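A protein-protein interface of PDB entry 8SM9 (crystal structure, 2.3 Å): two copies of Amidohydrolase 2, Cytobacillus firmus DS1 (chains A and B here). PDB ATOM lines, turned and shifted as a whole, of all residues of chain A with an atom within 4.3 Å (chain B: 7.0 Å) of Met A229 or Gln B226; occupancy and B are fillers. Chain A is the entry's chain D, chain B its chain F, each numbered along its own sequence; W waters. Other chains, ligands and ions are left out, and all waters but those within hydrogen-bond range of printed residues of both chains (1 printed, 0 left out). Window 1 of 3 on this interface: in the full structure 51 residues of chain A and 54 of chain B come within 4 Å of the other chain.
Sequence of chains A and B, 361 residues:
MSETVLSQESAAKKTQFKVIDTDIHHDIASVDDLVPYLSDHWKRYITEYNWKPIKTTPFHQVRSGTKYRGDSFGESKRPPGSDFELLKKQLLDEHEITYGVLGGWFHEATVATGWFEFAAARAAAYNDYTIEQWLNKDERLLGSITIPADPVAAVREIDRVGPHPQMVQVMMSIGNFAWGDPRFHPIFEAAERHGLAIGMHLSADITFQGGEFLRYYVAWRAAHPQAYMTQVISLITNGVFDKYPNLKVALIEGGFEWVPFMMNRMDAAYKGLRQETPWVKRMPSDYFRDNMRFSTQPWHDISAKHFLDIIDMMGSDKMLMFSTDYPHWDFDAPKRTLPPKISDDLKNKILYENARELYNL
O of Gln B226 sits close to OE1 of Gln A226, 3.1 Å away.
OE1 of Gln B209 lies within hydrogen-bond range of OG1 of Thr A230, at 3.3 Å.
The side-chain hydroxyl (OG1) of Thr A230 is in hydrogen-bond range of the side-chain amide oxygen (OE1) of Gln B226 (2.6 Å).
The side-chain hydroxyl (OG1) of Thr B230 sits at hydrogen-bond distance from the side-chain amide nitrogen (NE2) of Gln A226, at 2.9 Å.
The side-chain hydroxyl (OG1) of Thr A230 is in hydrogen-bond range of the backbone carbonyl oxygen (O) of Gln A226.
O of Gln B226 sits at hydrogen-bond distance from OG1 of Thr B230 (3.5 Å).
The backbone carbonyl oxygen (O) of Gly B254 is in hydrogen-bond range of the indole nitrogen (NE1) of Trp B258.
Among the printed residues, pairs that only touch across the chains: Phe A261 with Trp B258, Trp A258 with Phe B261, Met A229 with Gln B226, Phe A261 with Pro B225, Ile A233 with Ala B222, Ile A233 with Ala B219, Met A262 with Ala B222, Gln A226 with Met B229, Ile A233 with Ala B223, Ala A227 with Gln B209, Pro A225 with Phe B261, Phe A261 with Met B229 and Thr A230 with Leu B214.
Met A229 touches one residue of chain B.
Of the printed residues of chain A, Ala B222 touches Ile A233 (3.6 Å) and Met A262 (3.6 Å).
Of the printed residues of chain B, Ala A227 touches Gln B209 (3.7 Å).
The nearest residue of chain A that does not touch Gln B226 is Ile A233 (4.2 Å).
Printed residues of chain B that touch a printed residue of chain A: Gln B209, Leu B214, Ala B219, Ala B222, Ala B223, Pro B225, Gln B226, Met B229, Thr B230, Trp B258 and Phe B261.
Along chain B the printed residues that touch a printed residue of chain A span positions 209 to 261.
Of the 12 printed residues of chain A, 9 touch a printed residue of chain B.
Printed residues of chain A that touch a printed residue of chain B: Pro A225, Gln A226, Ala A227, Met A229, Thr A230, Ile A233, Trp A258, Phe A261 and Met A262.
Hydrophobic or aromatic side chains of chain A within 4 Å of the printed part of chain B: Pro A225, Ala A227, Met A229, Ile A233, Trp A258, Phe A261 and Met A262.
Among the printed residues, no Asp or Glu carboxylate lies within 4 Å of a Lys or Arg side-chain nitrogen of the other chain.
Pro A225 touches Phe B261, and with the chains exchanged Phe A261 touches Pro B225.
Gln A226 touches its own counterpart, Gln B226.
Gln A226 touches Thr B230, and with the chains exchanged Thr A230 touches Gln B226.
Phe A261 touches Met B229, but with the chains exchanged Met A229 does not touch Phe B261 (5.4 Å).
Positions printed for both chains: 225, 226, 227, 228, 229, 230, 231, 233, 258 and 261.
Water W1 lies within hydrogen-bond range of the side-chain amide nitrogen (NE2) of Gln A231 (2.9 Å) and the side-chain amide oxygen (OE1) of Gln B209 (3.2 Å).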
ATOM      1  N   PRO A 225      35.064  -2.733   8.584  1.00  0.00           N
ATOM      2  CA  PRO A 225      35.107  -3.409   7.271  1.00  0.00           C
ATOM      3  C   PRO A 225      34.446  -2.616   6.147  1.00  0.00           C
ATOM      4  O   PRO A 225      34.790  -2.791   4.969  1.00  0.00           O
ATOM      5  CB  PRO A 225      34.370  -4.718   7.542  1.00  0.00           C
ATOM      6  CG  PRO A 225      34.725  -5.016   8.979  1.00  0.00           C
ATOM      7  CD  PRO A 225      34.743  -3.694   9.667  1.00  0.00           C
ATOM      8  N   GLN A 226      33.512  -1.722   6.502  1.00  0.00           N
ATOM      9  CA  GLN A 226      32.905  -0.816   5.520  1.00  0.00           C
ATOM     10  C   GLN A 226      33.960  -0.018   4.759  1.00  0.00           C
ATOM     11  O   GLN A 226      33.870   0.135   3.533  1.00  0.00           O
ATOM     12  CB  GLN A 226      31.938   0.142   6.209  1.00  0.00           C
ATOM     13  CG  GLN A 226      30.674  -0.484   6.790  1.00  0.00           C
ATOM     14  CD  GLN A 226      29.899   0.507   7.646  1.00  0.00           C
ATOM     15  OE1 GLN A 226      29.762   1.682   7.288  1.00  0.00           O
ATOM     16  NE2 GLN A 226      29.399   0.046   8.779  1.00  0.00           N
ATOM     17  N   ALA A 227      34.973   0.494   5.463  1.00  0.00           N
ATOM     18  CA  ALA A 227      36.036   1.225   4.776  1.00  0.00           C
ATOM     19  C   ALA A 227      36.786   0.331   3.790  1.00  0.00           C
ATOM     20  O   ALA A 227      37.144   0.780   2.693  1.00  0.00           O
ATOM     21  CB  ALA A 227      36.994   1.843   5.795  1.00  0.00           C
ATOM     22  N   TYR A 228      37.037  -0.932   4.160  1.00  0.00           N
ATOM     23  CA  TYR A 228      37.604  -1.883   3.200  1.00  0.00           C
ATOM     24  C   TYR A 228      36.704  -2.007   1.977  1.00  0.00           C
ATOM     25  O   TYR A 228      37.163  -1.896   0.835  1.00  0.00           O
ATOM     26  CB  TYR A 228      37.822  -3.263   3.856  1.00  0.00           C
ATOM     27  CG  TYR A 228      39.005  -3.312   4.830  1.00  0.00           C
ATOM     28  CD1 TYR A 228      38.892  -2.798   6.116  1.00  0.00           C
ATOM     29  CD2 TYR A 228      40.225  -3.847   4.458  1.00  0.00           C
ATOM     30  CE1 TYR A 228      39.948  -2.830   7.008  1.00  0.00           C
ATOM     31  CE2 TYR A 228      41.298  -3.868   5.351  1.00  0.00           C
ATOM     32  CZ  TYR A 228      41.144  -3.362   6.627  1.00  0.00           C
ATOM     33  OH  TYR A 228      42.182  -3.383   7.525  1.00  0.00           O
ATOM     34  N   MET A 229      35.404  -2.196   2.208  1.00  0.00           N
ATOM     35  CA  MET A 229      34.464  -2.331   1.105  1.00  0.00           C
ATOM     36  C   MET A 229      34.490  -1.121   0.181  1.00  0.00           C
ATOM     37  O   MET A 229      34.425  -1.287  -1.044  1.00  0.00           O
ATOM     38  CB  MET A 229      33.053  -2.549   1.638  1.00  0.00           C
ATOM     39  CG  MET A 229      32.891  -3.761   2.519  1.00  0.00           C
ATOM     40  SD  MET A 229      31.220  -3.888   3.143  1.00  0.00           S
ATOM     41  CE  MET A 229      30.433  -2.856   1.907  1.00  0.00           C
ATOM     42  N   THR A 230      34.610   0.075   0.747  1.00  0.00           N
ATOM     43  CA  THR A 230      34.679   1.311  -0.064  1.00  0.00           C
ATOM     44  C   THR A 230      35.929   1.263  -0.952  1.00  0.00           C
ATOM     45  O   THR A 230      35.835   1.696  -2.103  1.00  0.00           O
ATOM     46  CB  THR A 230      34.605   2.559   0.825  1.00  0.00           C
ATOM     47  OG1 THR A 230      33.302   2.632   1.399  1.00  0.00           O
ATOM     48  CG2 THR A 230      34.907   3.837   0.076  1.00  0.00           C
ATOM     49  N   GLN A 231      37.038   0.731  -0.445  1.00  0.00           N
ATOM     50  CA  GLN A 231      38.257   0.759  -1.255  1.00  0.00           C
ATOM     51  C   GLN A 231      38.147  -0.184  -2.455  1.00  0.00           C
ATOM     52  O   GLN A 231      38.610   0.145  -3.558  1.00  0.00           O
ATOM     53  CB  GLN A 231      39.481   0.430  -0.410  1.00  0.00           C
ATOM     54  CG  GLN A 231      39.635   1.325   0.838  1.00  0.00           C
ATOM     55  CD  GLN A 231      40.002   2.790   0.538  1.00  0.00           C
ATOM     56  OE1 GLN A 231      40.582   3.105  -0.501  1.00  0.00           O
ATOM     57  NE2 GLN A 231      39.684   3.680   1.473  1.00  0.00           N
ATOM     58  N   VAL A 232      37.517  -1.354  -2.284  1.00  0.00           N
ATOM     59  CA  VAL A 232      37.392  -2.254  -3.433  1.00  0.00           C
ATOM     60  C   VAL A 232      36.458  -1.651  -4.482  1.00  0.00           C
ATOM     61  O   VAL A 232      36.750  -1.681  -5.684  1.00  0.00           O
ATOM     62  CB  VAL A 232      36.968  -3.672  -2.994  1.00  0.00           C
ATOM     63  CG1 VAL A 232      37.853  -4.158  -1.856  1.00  0.00           C
ATOM     64  CG2 VAL A 232      35.493  -3.780  -2.611  1.00  0.00           C
ATOM     65  N   ILE A 233      35.364  -1.030  -4.047  1.00  0.00           N
ATOM     66  CA  ILE A 233      34.520  -0.274  -4.968  1.00  0.00           C
ATOM     67  C   ILE A 233      35.337   0.808  -5.664  1.00  0.00           C
ATOM     68  O   ILE A 233      35.242   1.012  -6.881  1.00  0.00           O
ATOM     69  CB  ILE A 233      33.326   0.329  -4.202  1.00  0.00           C
ATOM     70  CG1 ILE A 233      32.511  -0.766  -3.487  1.00  0.00           C
ATOM     71  CG2 ILE A 233      32.471   1.202  -5.134  1.00  0.00           C
ATOM     72  CD1 ILE A 233      31.492  -0.222  -2.480  1.00  0.00           C
ATOM     73  N   TRP A 258      32.093 -10.865   3.964  1.00  0.00           N
ATOM     74  CA  TRP A 258      31.309  -9.933   3.169  1.00  0.00           C
ATOM     75  C   TRP A 258      31.673  -9.958   1.697  1.00  0.00           C
ATOM     76  O   TRP A 258      31.054  -9.236   0.913  1.00  0.00           O
ATOM     77  CB  TRP A 258      31.498  -8.507   3.687  1.00  0.00           C
ATOM     78  CG  TRP A 258      32.973  -8.068   3.807  1.00  0.00           C
ATOM     79  CD1 TRP A 258      33.766  -8.173   4.917  1.00  0.00           C
ATOM     80  CD2 TRP A 258      33.795  -7.460   2.790  1.00  0.00           C
ATOM     81  NE1 TRP A 258      35.025  -7.672   4.658  1.00  0.00           N
ATOM     82  CE2 TRP A 258      35.075  -7.234   3.362  1.00  0.00           C
ATOM     83  CE3 TRP A 258      33.578  -7.085   1.463  1.00  0.00           C
ATOM     84  CZ2 TRP A 258      36.133  -6.654   2.653  1.00  0.00           C
ATOM     85  CZ3 TRP A 258      34.640  -6.495   0.748  1.00  0.00           C
ATOM     86  CH2 TRP A 258      35.901  -6.290   1.352  1.00  0.00           C
ATOM     87  N   PHE A 261      29.028 -10.957  -0.999  1.00  0.00           N
ATOM     88  CA  PHE A 261      27.992  -9.941  -1.088  1.00  0.00           C
ATOM     89  C   PHE A 261      28.428  -8.793  -2.001  1.00  0.00           C
ATOM     90  O   PHE A 261      27.689  -8.400  -2.917  1.00  0.00           O
ATOM     91  CB  PHE A 261      27.653  -9.457   0.318  1.00  0.00           C
ATOM     92  CG  PHE A 261      27.216  -8.051   0.371  1.00  0.00           C
ATOM     93  CD1 PHE A 261      25.934  -7.696  -0.041  1.00  0.00           C
ATOM     94  CD2 PHE A 261      28.087  -7.061   0.821  1.00  0.00           C
ATOM     95  CE1 PHE A 261      25.519  -6.365   0.006  1.00  0.00           C
ATOM     96  CE2 PHE A 261      27.684  -5.720   0.874  1.00  0.00           C
ATOM     97  CZ  PHE A 261      26.408  -5.367   0.469  1.00  0.00           C
ATOM     98  N   MET A 262      29.650  -8.275  -1.798  1.00  0.00           N
ATOM     99  CA  MET A 262      30.156  -7.168  -2.617  1.00  0.00           C
ATOM    100  C   MET A 262      30.295  -7.561  -4.083  1.00  0.00           C
ATOM    101  O   MET A 262      29.954  -6.774  -4.980  1.00  0.00           O
ATOM    102  CB  MET A 262      31.507  -6.684  -2.081  1.00  0.00           C
ATOM    103  CG  MET A 262      31.446  -5.495  -1.116  1.00  0.00           C
ATOM    104  SD  MET A 262      30.054  -4.360  -1.352  1.00  0.00           S
ATOM    105  CE  MET A 262      30.441  -3.706  -2.960  1.00  0.00           C
ATOM    106  N   ILE B 206      23.234   9.970   1.495  1.00  0.00           N
ATOM    107  CA  ILE B 206      24.283   9.221   2.198  1.00  0.00           C
ATOM    108  C   ILE B 206      25.649   9.487   1.565  1.00  0.00           C
ATOM    109  O   ILE B 206      25.802   9.455   0.336  1.00  0.00           O
ATOM    110  CB  ILE B 206      23.954   7.725   2.165  1.00  0.00           C
ATOM    111  CG1 ILE B 206      22.619   7.449   2.853  1.00  0.00           C
ATOM    112  CG2 ILE B 206      25.046   6.918   2.830  1.00  0.00           C
ATOM    113  CD1 ILE B 206      22.090   5.988   2.639  1.00  0.00           C
ATOM    114  N   THR B 207      26.658   9.741   2.401  1.00  0.00           N
ATOM    115  CA  THR B 207      28.056   9.730   1.959  1.00  0.00           C
ATOM    116  C   THR B 207      28.834   8.664   2.762  1.00  0.00           C
ATOM    117  O   THR B 207      28.250   7.888   3.524  1.00  0.00           O
ATOM    118  CB  THR B 207      28.683  11.129   2.061  1.00  0.00           C
ATOM    119  OG1 THR B 207      28.543  11.637   3.385  1.00  0.00           O
ATOM    120  CG2 THR B 207      27.993  12.078   1.152  1.00  0.00           C
ATOM    121  N   PHE B 208      30.159   8.615   2.578  1.00  0.00           N
ATOM    122  CA  PHE B 208      30.977   7.612   3.255  1.00  0.00           C
ATOM    123  C   PHE B 208      32.205   8.276   3.874  1.00  0.00           C
ATOM    124  O   PHE B 208      32.124   9.442   4.271  1.00  0.00           O
ATOM    125  CB  PHE B 208      31.316   6.467   2.276  1.00  0.00           C
ATOM    126  CG  PHE B 208      30.087   5.904   1.618  1.00  0.00           C
ATOM    127  CD1 PHE B 208      29.275   5.012   2.302  1.00  0.00           C
ATOM    128  CD2 PHE B 208      29.667   6.363   0.373  1.00  0.00           C
ATOM    129  CE1 PHE B 208      28.090   4.527   1.735  1.00  0.00           C
ATOM    130  CE2 PHE B 208      28.486   5.890  -0.196  1.00  0.00           C
ATOM    131  CZ  PHE B 208      27.698   4.972   0.489  1.00  0.00           C
ATOM    132  N   GLN B 209      33.323   7.554   3.990  1.00  0.00           N
ATOM    133  CA  GLN B 209      34.508   8.087   4.666  1.00  0.00           C
ATOM    134  C   GLN B 209      34.958   9.401   4.044  1.00  0.00           C
ATOM    135  O   GLN B 209      35.014   9.545   2.821  1.00  0.00           O
ATOM    136  CB  GLN B 209      35.654   7.074   4.612  1.00  0.00           C
ATOM    137  CG  GLN B 209      35.466   5.879   5.552  1.00  0.00           C
ATOM    138  CD  GLN B 209      34.556   4.827   4.963  1.00  0.00           C
ATOM    139  OE1 GLN B 209      34.626   4.526   3.764  1.00  0.00           O
ATOM    140  NE2 GLN B 209      33.674   4.276   5.796  1.00  0.00           N
ATOM    141  N   LEU B 214      32.079   9.194  -3.905  1.00  0.00           N
ATOM    142  CA  LEU B 214      32.724   8.122  -4.674  1.00  0.00           C
ATOM    143  C   LEU B 214      32.543   8.264  -6.188  1.00  0.00           C
ATOM    144  O   LEU B 214      32.479   7.246  -6.889  1.00  0.00           O
ATOM    145  CB  LEU B 214      32.223   6.722  -4.233  1.00  0.00           C
ATOM    146  CG  LEU B 214      32.284   6.404  -2.728  1.00  0.00           C
ATOM    147  CD1 LEU B 214      31.920   4.966  -2.377  1.00  0.00           C
ATOM    148  CD2 LEU B 214      33.653   6.747  -2.195  1.00  0.00           C
ATOM    149  N   ALA B 219      29.365   3.480  -8.212  1.00  0.00           N
ATOM    150  CA  ALA B 219      30.059   3.253  -6.947  1.00  0.00           C
ATOM    151  C   ALA B 219      29.157   3.536  -5.746  1.00  0.00           C
ATOM    152  O   ALA B 219      29.157   2.777  -4.767  1.00  0.00           O
ATOM    153  CB  ALA B 219      31.314   4.119  -6.876  1.00  0.00           C
ATOM    154  N   ALA B 222      26.896   0.830  -5.054  1.00  0.00           N
ATOM    155  CA  ALA B 222      27.607  -0.298  -4.473  1.00  0.00           C
ATOM    156  C   ALA B 222      27.880  -0.113  -2.985  1.00  0.00           C
ATOM    157  O   ALA B 222      28.034  -1.097  -2.264  1.00  0.00           O
ATOM    158  CB  ALA B 222      28.920  -0.497  -5.220  1.00  0.00           C
ATOM    159  N   ALA B 223      27.960   1.131  -2.506  1.00  0.00           N
ATOM    160  CA  ALA B 223      28.415   1.364  -1.147  1.00  0.00           C
ATOM    161  C   ALA B 223      27.293   1.594  -0.156  1.00  0.00           C
ATOM    162  O   ALA B 223      27.484   1.300   1.026  1.00  0.00           O
ATOM    163  CB  ALA B 223      29.383   2.549  -1.082  1.00  0.00           C
ATOM    164  N   HIS B 224      26.120   2.044  -0.585  1.00  0.00           N
ATOM    165  CA  HIS B 224      25.200   2.457   0.468  1.00  0.00           C
ATOM    166  C   HIS B 224      24.657   1.338   1.359  1.00  0.00           C
ATOM    167  O   HIS B 224      24.020   1.657   2.367  1.00  0.00           O
ATOM    168  CB  HIS B 224      24.040   3.288  -0.100  1.00  0.00           C
ATOM    169  CG  HIS B 224      23.033   2.517  -0.891  1.00  0.00           C
ATOM    170  ND1 HIS B 224      22.609   2.928  -2.138  1.00  0.00           N
ATOM    171  CD2 HIS B 224      22.321   1.402  -0.603  1.00  0.00           C
ATOM    172  CE1 HIS B 224      21.710   2.076  -2.603  1.00  0.00           C
ATOM    173  NE2 HIS B 224      21.521   1.136  -1.692  1.00  0.00           N
ATOM    174  N   PRO B 225      24.851   0.039   1.075  1.00  0.00           N
ATOM    175  CA  PRO B 225      24.562  -0.945   2.135  1.00  0.00           C
ATOM    176  C   PRO B 225      25.348  -0.708   3.410  1.00  0.00           C
ATOM    177  O   PRO B 225      24.831  -1.022   4.489  1.00  0.00           O
ATOM    178  CB  PRO B 225      24.919  -2.280   1.478  1.00  0.00           C
ATOM    179  CG  PRO B 225      24.535  -2.052   0.096  1.00  0.00           C
ATOM    180  CD  PRO B 225      24.915  -0.644  -0.237  1.00  0.00           C
ATOM    181  N   GLN B 226      26.564  -0.147   3.317  1.00  0.00           N
ATOM    182  CA  GLN B 226      27.367   0.187   4.497  1.00  0.00           C
ATOM    183  C   GLN B 226      26.580   1.007   5.512  1.00  0.00           C
ATOM    184  O   GLN B 226      26.781   0.865   6.722  1.00  0.00           O
ATOM    185  CB  GLN B 226      28.613   0.984   4.085  1.00  0.00           C
ATOM    186  CG  GLN B 226      29.575   0.300   3.143  1.00  0.00           C
ATOM    187  CD  GLN B 226      30.683   1.228   2.645  1.00  0.00           C
ATOM    188  OE1 GLN B 226      31.155   1.084   1.506  1.00  0.00           O
ATOM    189  NE2 GLN B 226      31.091   2.201   3.489  1.00  0.00           N
ATOM    190  N   ALA B 227      25.741   1.933   5.037  1.00  0.00           N
ATOM    191  CA  ALA B 227      25.000   2.767   5.967  1.00  0.00           C
ATOM    192  C   ALA B 227      23.949   1.962   6.702  1.00  0.00           C
ATOM    193  O   ALA B 227      23.668   2.245   7.866  1.00  0.00           O
ATOM    194  CB  ALA B 227      24.353   3.936   5.232  1.00  0.00           C
ATOM    195  N   TYR B 228      23.362   0.962   6.036  1.00  0.00           N
ATOM    196  CA  TYR B 228      22.488   0.020   6.719  1.00  0.00           C
ATOM    197  C   TYR B 228      23.253  -0.722   7.799  1.00  0.00           C
ATOM    198  O   TYR B 228      22.731  -0.968   8.893  1.00  0.00           O
ATOM    199  CB  TYR B 228      21.906  -0.971   5.718  1.00  0.00           C
ATOM    200  CG  TYR B 228      20.838  -0.398   4.828  1.00  0.00           C
ATOM    201  CD1 TYR B 228      21.165   0.449   3.766  1.00  0.00           C
ATOM    202  CD2 TYR B 228      19.493  -0.712   5.034  1.00  0.00           C
ATOM    203  CE1 TYR B 228      20.192   0.965   2.931  1.00  0.00           C
ATOM    204  CE2 TYR B 228      18.503  -0.186   4.204  1.00  0.00           C
ATOM    205  CZ  TYR B 228      18.868   0.642   3.155  1.00  0.00           C
ATOM    206  OH  TYR B 228      17.901   1.142   2.336  1.00  0.00           O
ATOM    207  N   MET B 229      24.513  -1.035   7.510  1.00  0.00           N
ATOM    208  CA  MET B 229      25.360  -1.779   8.422  1.00  0.00           C
ATOM    209  C   MET B 229      25.625  -0.982   9.692  1.00  0.00           C
ATOM    210  O   MET B 229      25.661  -1.543  10.791  1.00  0.00           O
ATOM    211  CB  MET B 229      26.670  -2.118   7.703  1.00  0.00           C
ATOM    212  CG  MET B 229      26.738  -3.504   7.102  1.00  0.00           C
ATOM    213  SD  MET B 229      28.016  -3.592   5.808  1.00  0.00           S
ATOM    214  CE  MET B 229      27.094  -4.167   4.386  1.00  0.00           C
ATOM    215  N   THR B 230      25.778   0.315   9.556  1.00  0.00           N
ATOM    216  CA  THR B 230      26.038   1.153  10.694  1.00  0.00           C
ATOM    217  C   THR B 230      24.778   1.310  11.522  1.00  0.00           C
ATOM    218  O   THR B 230      24.834   1.391  12.734  1.00  0.00           O
ATOM    219  CB  THR B 230      26.590   2.520  10.239  1.00  0.00           C
ATOM    220  OG1 THR B 230      27.893   2.344   9.679  1.00  0.00           O
ATOM    221  CG2 THR B 230      26.672   3.488  11.395  1.00  0.00           C
ATOM    222  N   GLN B 231      23.637   1.323  10.857  1.00  0.00           N
ATOM    223  CA  GLN B 231      22.397   1.478  11.610  1.00  0.00           C
ATOM    224  C   GLN B 231      22.167   0.277  12.523  1.00  0.00           C
ATOM    225  O   GLN B 231      21.825   0.451  13.699  1.00  0.00           O
ATOM    226  CB  GLN B 231      21.197   1.688  10.684  1.00  0.00           C
ATOM    227  CG  GLN B 231      21.196   2.976   9.834  1.00  0.00           C
ATOM    228  CD  GLN B 231      21.369   4.271  10.636  1.00  0.00           C
ATOM    229  OE1 GLN B 231      20.703   4.496  11.640  1.00  0.00           O
ATOM    230  NE2 GLN B 231      22.257   5.140  10.164  1.00  0.00           N
ATOM    231  N   ILE B 233      24.426  -1.872  13.685  1.00  0.00           N
ATOM    232  CA  ILE B 233      25.428  -1.785  14.746  1.00  0.00           C
ATOM    233  C   ILE B 233      24.970  -0.794  15.804  1.00  0.00           C
ATOM    234  O   ILE B 233      25.037  -1.048  17.011  1.00  0.00           O
ATOM    235  CB  ILE B 233      26.795  -1.365  14.166  1.00  0.00           C
ATOM    236  CG1 ILE B 233      27.412  -2.464  13.315  1.00  0.00           C
ATOM    237  CG2 ILE B 233      27.777  -0.988  15.271  1.00  0.00           C
ATOM    238  CD1 ILE B 233      28.461  -1.952  12.317  1.00  0.00           C
ATOM    239  N   GLY B 254      18.644  -2.388   1.740  1.00  0.00           N
ATOM    240  CA  GLY B 254      20.075  -2.441   1.917  1.00  0.00           C
ATOM    241  C   GLY B 254      20.679  -3.769   1.531  1.00  0.00           C
ATOM    242  O   GLY B 254      21.885  -3.969   1.715  1.00  0.00           O
ATOM    243  N   TRP B 258      24.826  -9.735   3.299  1.00  0.00           N
ATOM    244  CA  TRP B 258      25.854  -9.333   4.251  1.00  0.00           C
ATOM    245  C   TRP B 258      25.413  -9.522   5.686  1.00  0.00           C
ATOM    246  O   TRP B 258      26.214  -9.286   6.605  1.00  0.00           O
ATOM    247  CB  TRP B 258      26.198  -7.867   4.043  1.00  0.00           C
ATOM    248  CG  TRP B 258      24.979  -6.958   4.152  1.00  0.00           C
ATOM    249  CD1 TRP B 258      24.241  -6.463   3.116  1.00  0.00           C
ATOM    250  CD2 TRP B 258      24.363  -6.449   5.358  1.00  0.00           C
ATOM    251  NE1 TRP B 258      23.210  -5.674   3.594  1.00  0.00           N
ATOM    252  CE2 TRP B 258      23.266  -5.647   4.964  1.00  0.00           C
ATOM    253  CE3 TRP B 258      24.643  -6.575   6.726  1.00  0.00           C
ATOM    254  CZ2 TRP B 258      22.448  -4.973   5.890  1.00  0.00           C
ATOM    255  CZ3 TRP B 258      23.811  -5.911   7.646  1.00  0.00           C
ATOM    256  CH2 TRP B 258      22.734  -5.120   7.217  1.00  0.00           C
ATOM    257  N   PHE B 261      27.589 -12.064   7.722  1.00  0.00           N
ATOM    258  CA  PHE B 261      28.940 -11.554   8.080  1.00  0.00           C
ATOM    259  C   PHE B 261      28.860 -10.619   9.282  1.00  0.00           C
ATOM    260  O   PHE B 261      29.762 -10.651  10.117  1.00  0.00           O
ATOM    261  CB  PHE B 261      29.563 -10.826   6.888  1.00  0.00           C
ATOM    262  CG  PHE B 261      30.191  -9.493   7.197  1.00  0.00           C
ATOM    263  CD1 PHE B 261      31.487  -9.412   7.674  1.00  0.00           C
ATOM    264  CD2 PHE B 261      29.486  -8.317   7.004  1.00  0.00           C
ATOM    265  CE1 PHE B 261      32.063  -8.186   7.958  1.00  0.00           C
ATOM    266  CE2 PHE B 261      30.063  -7.091   7.289  1.00  0.00           C
ATOM    267  CZ  PHE B 261      31.351  -7.028   7.764  1.00  0.00           C
HETATM  268  O   HOH W   1      37.765   4.862   3.334  1.00  0.00           O
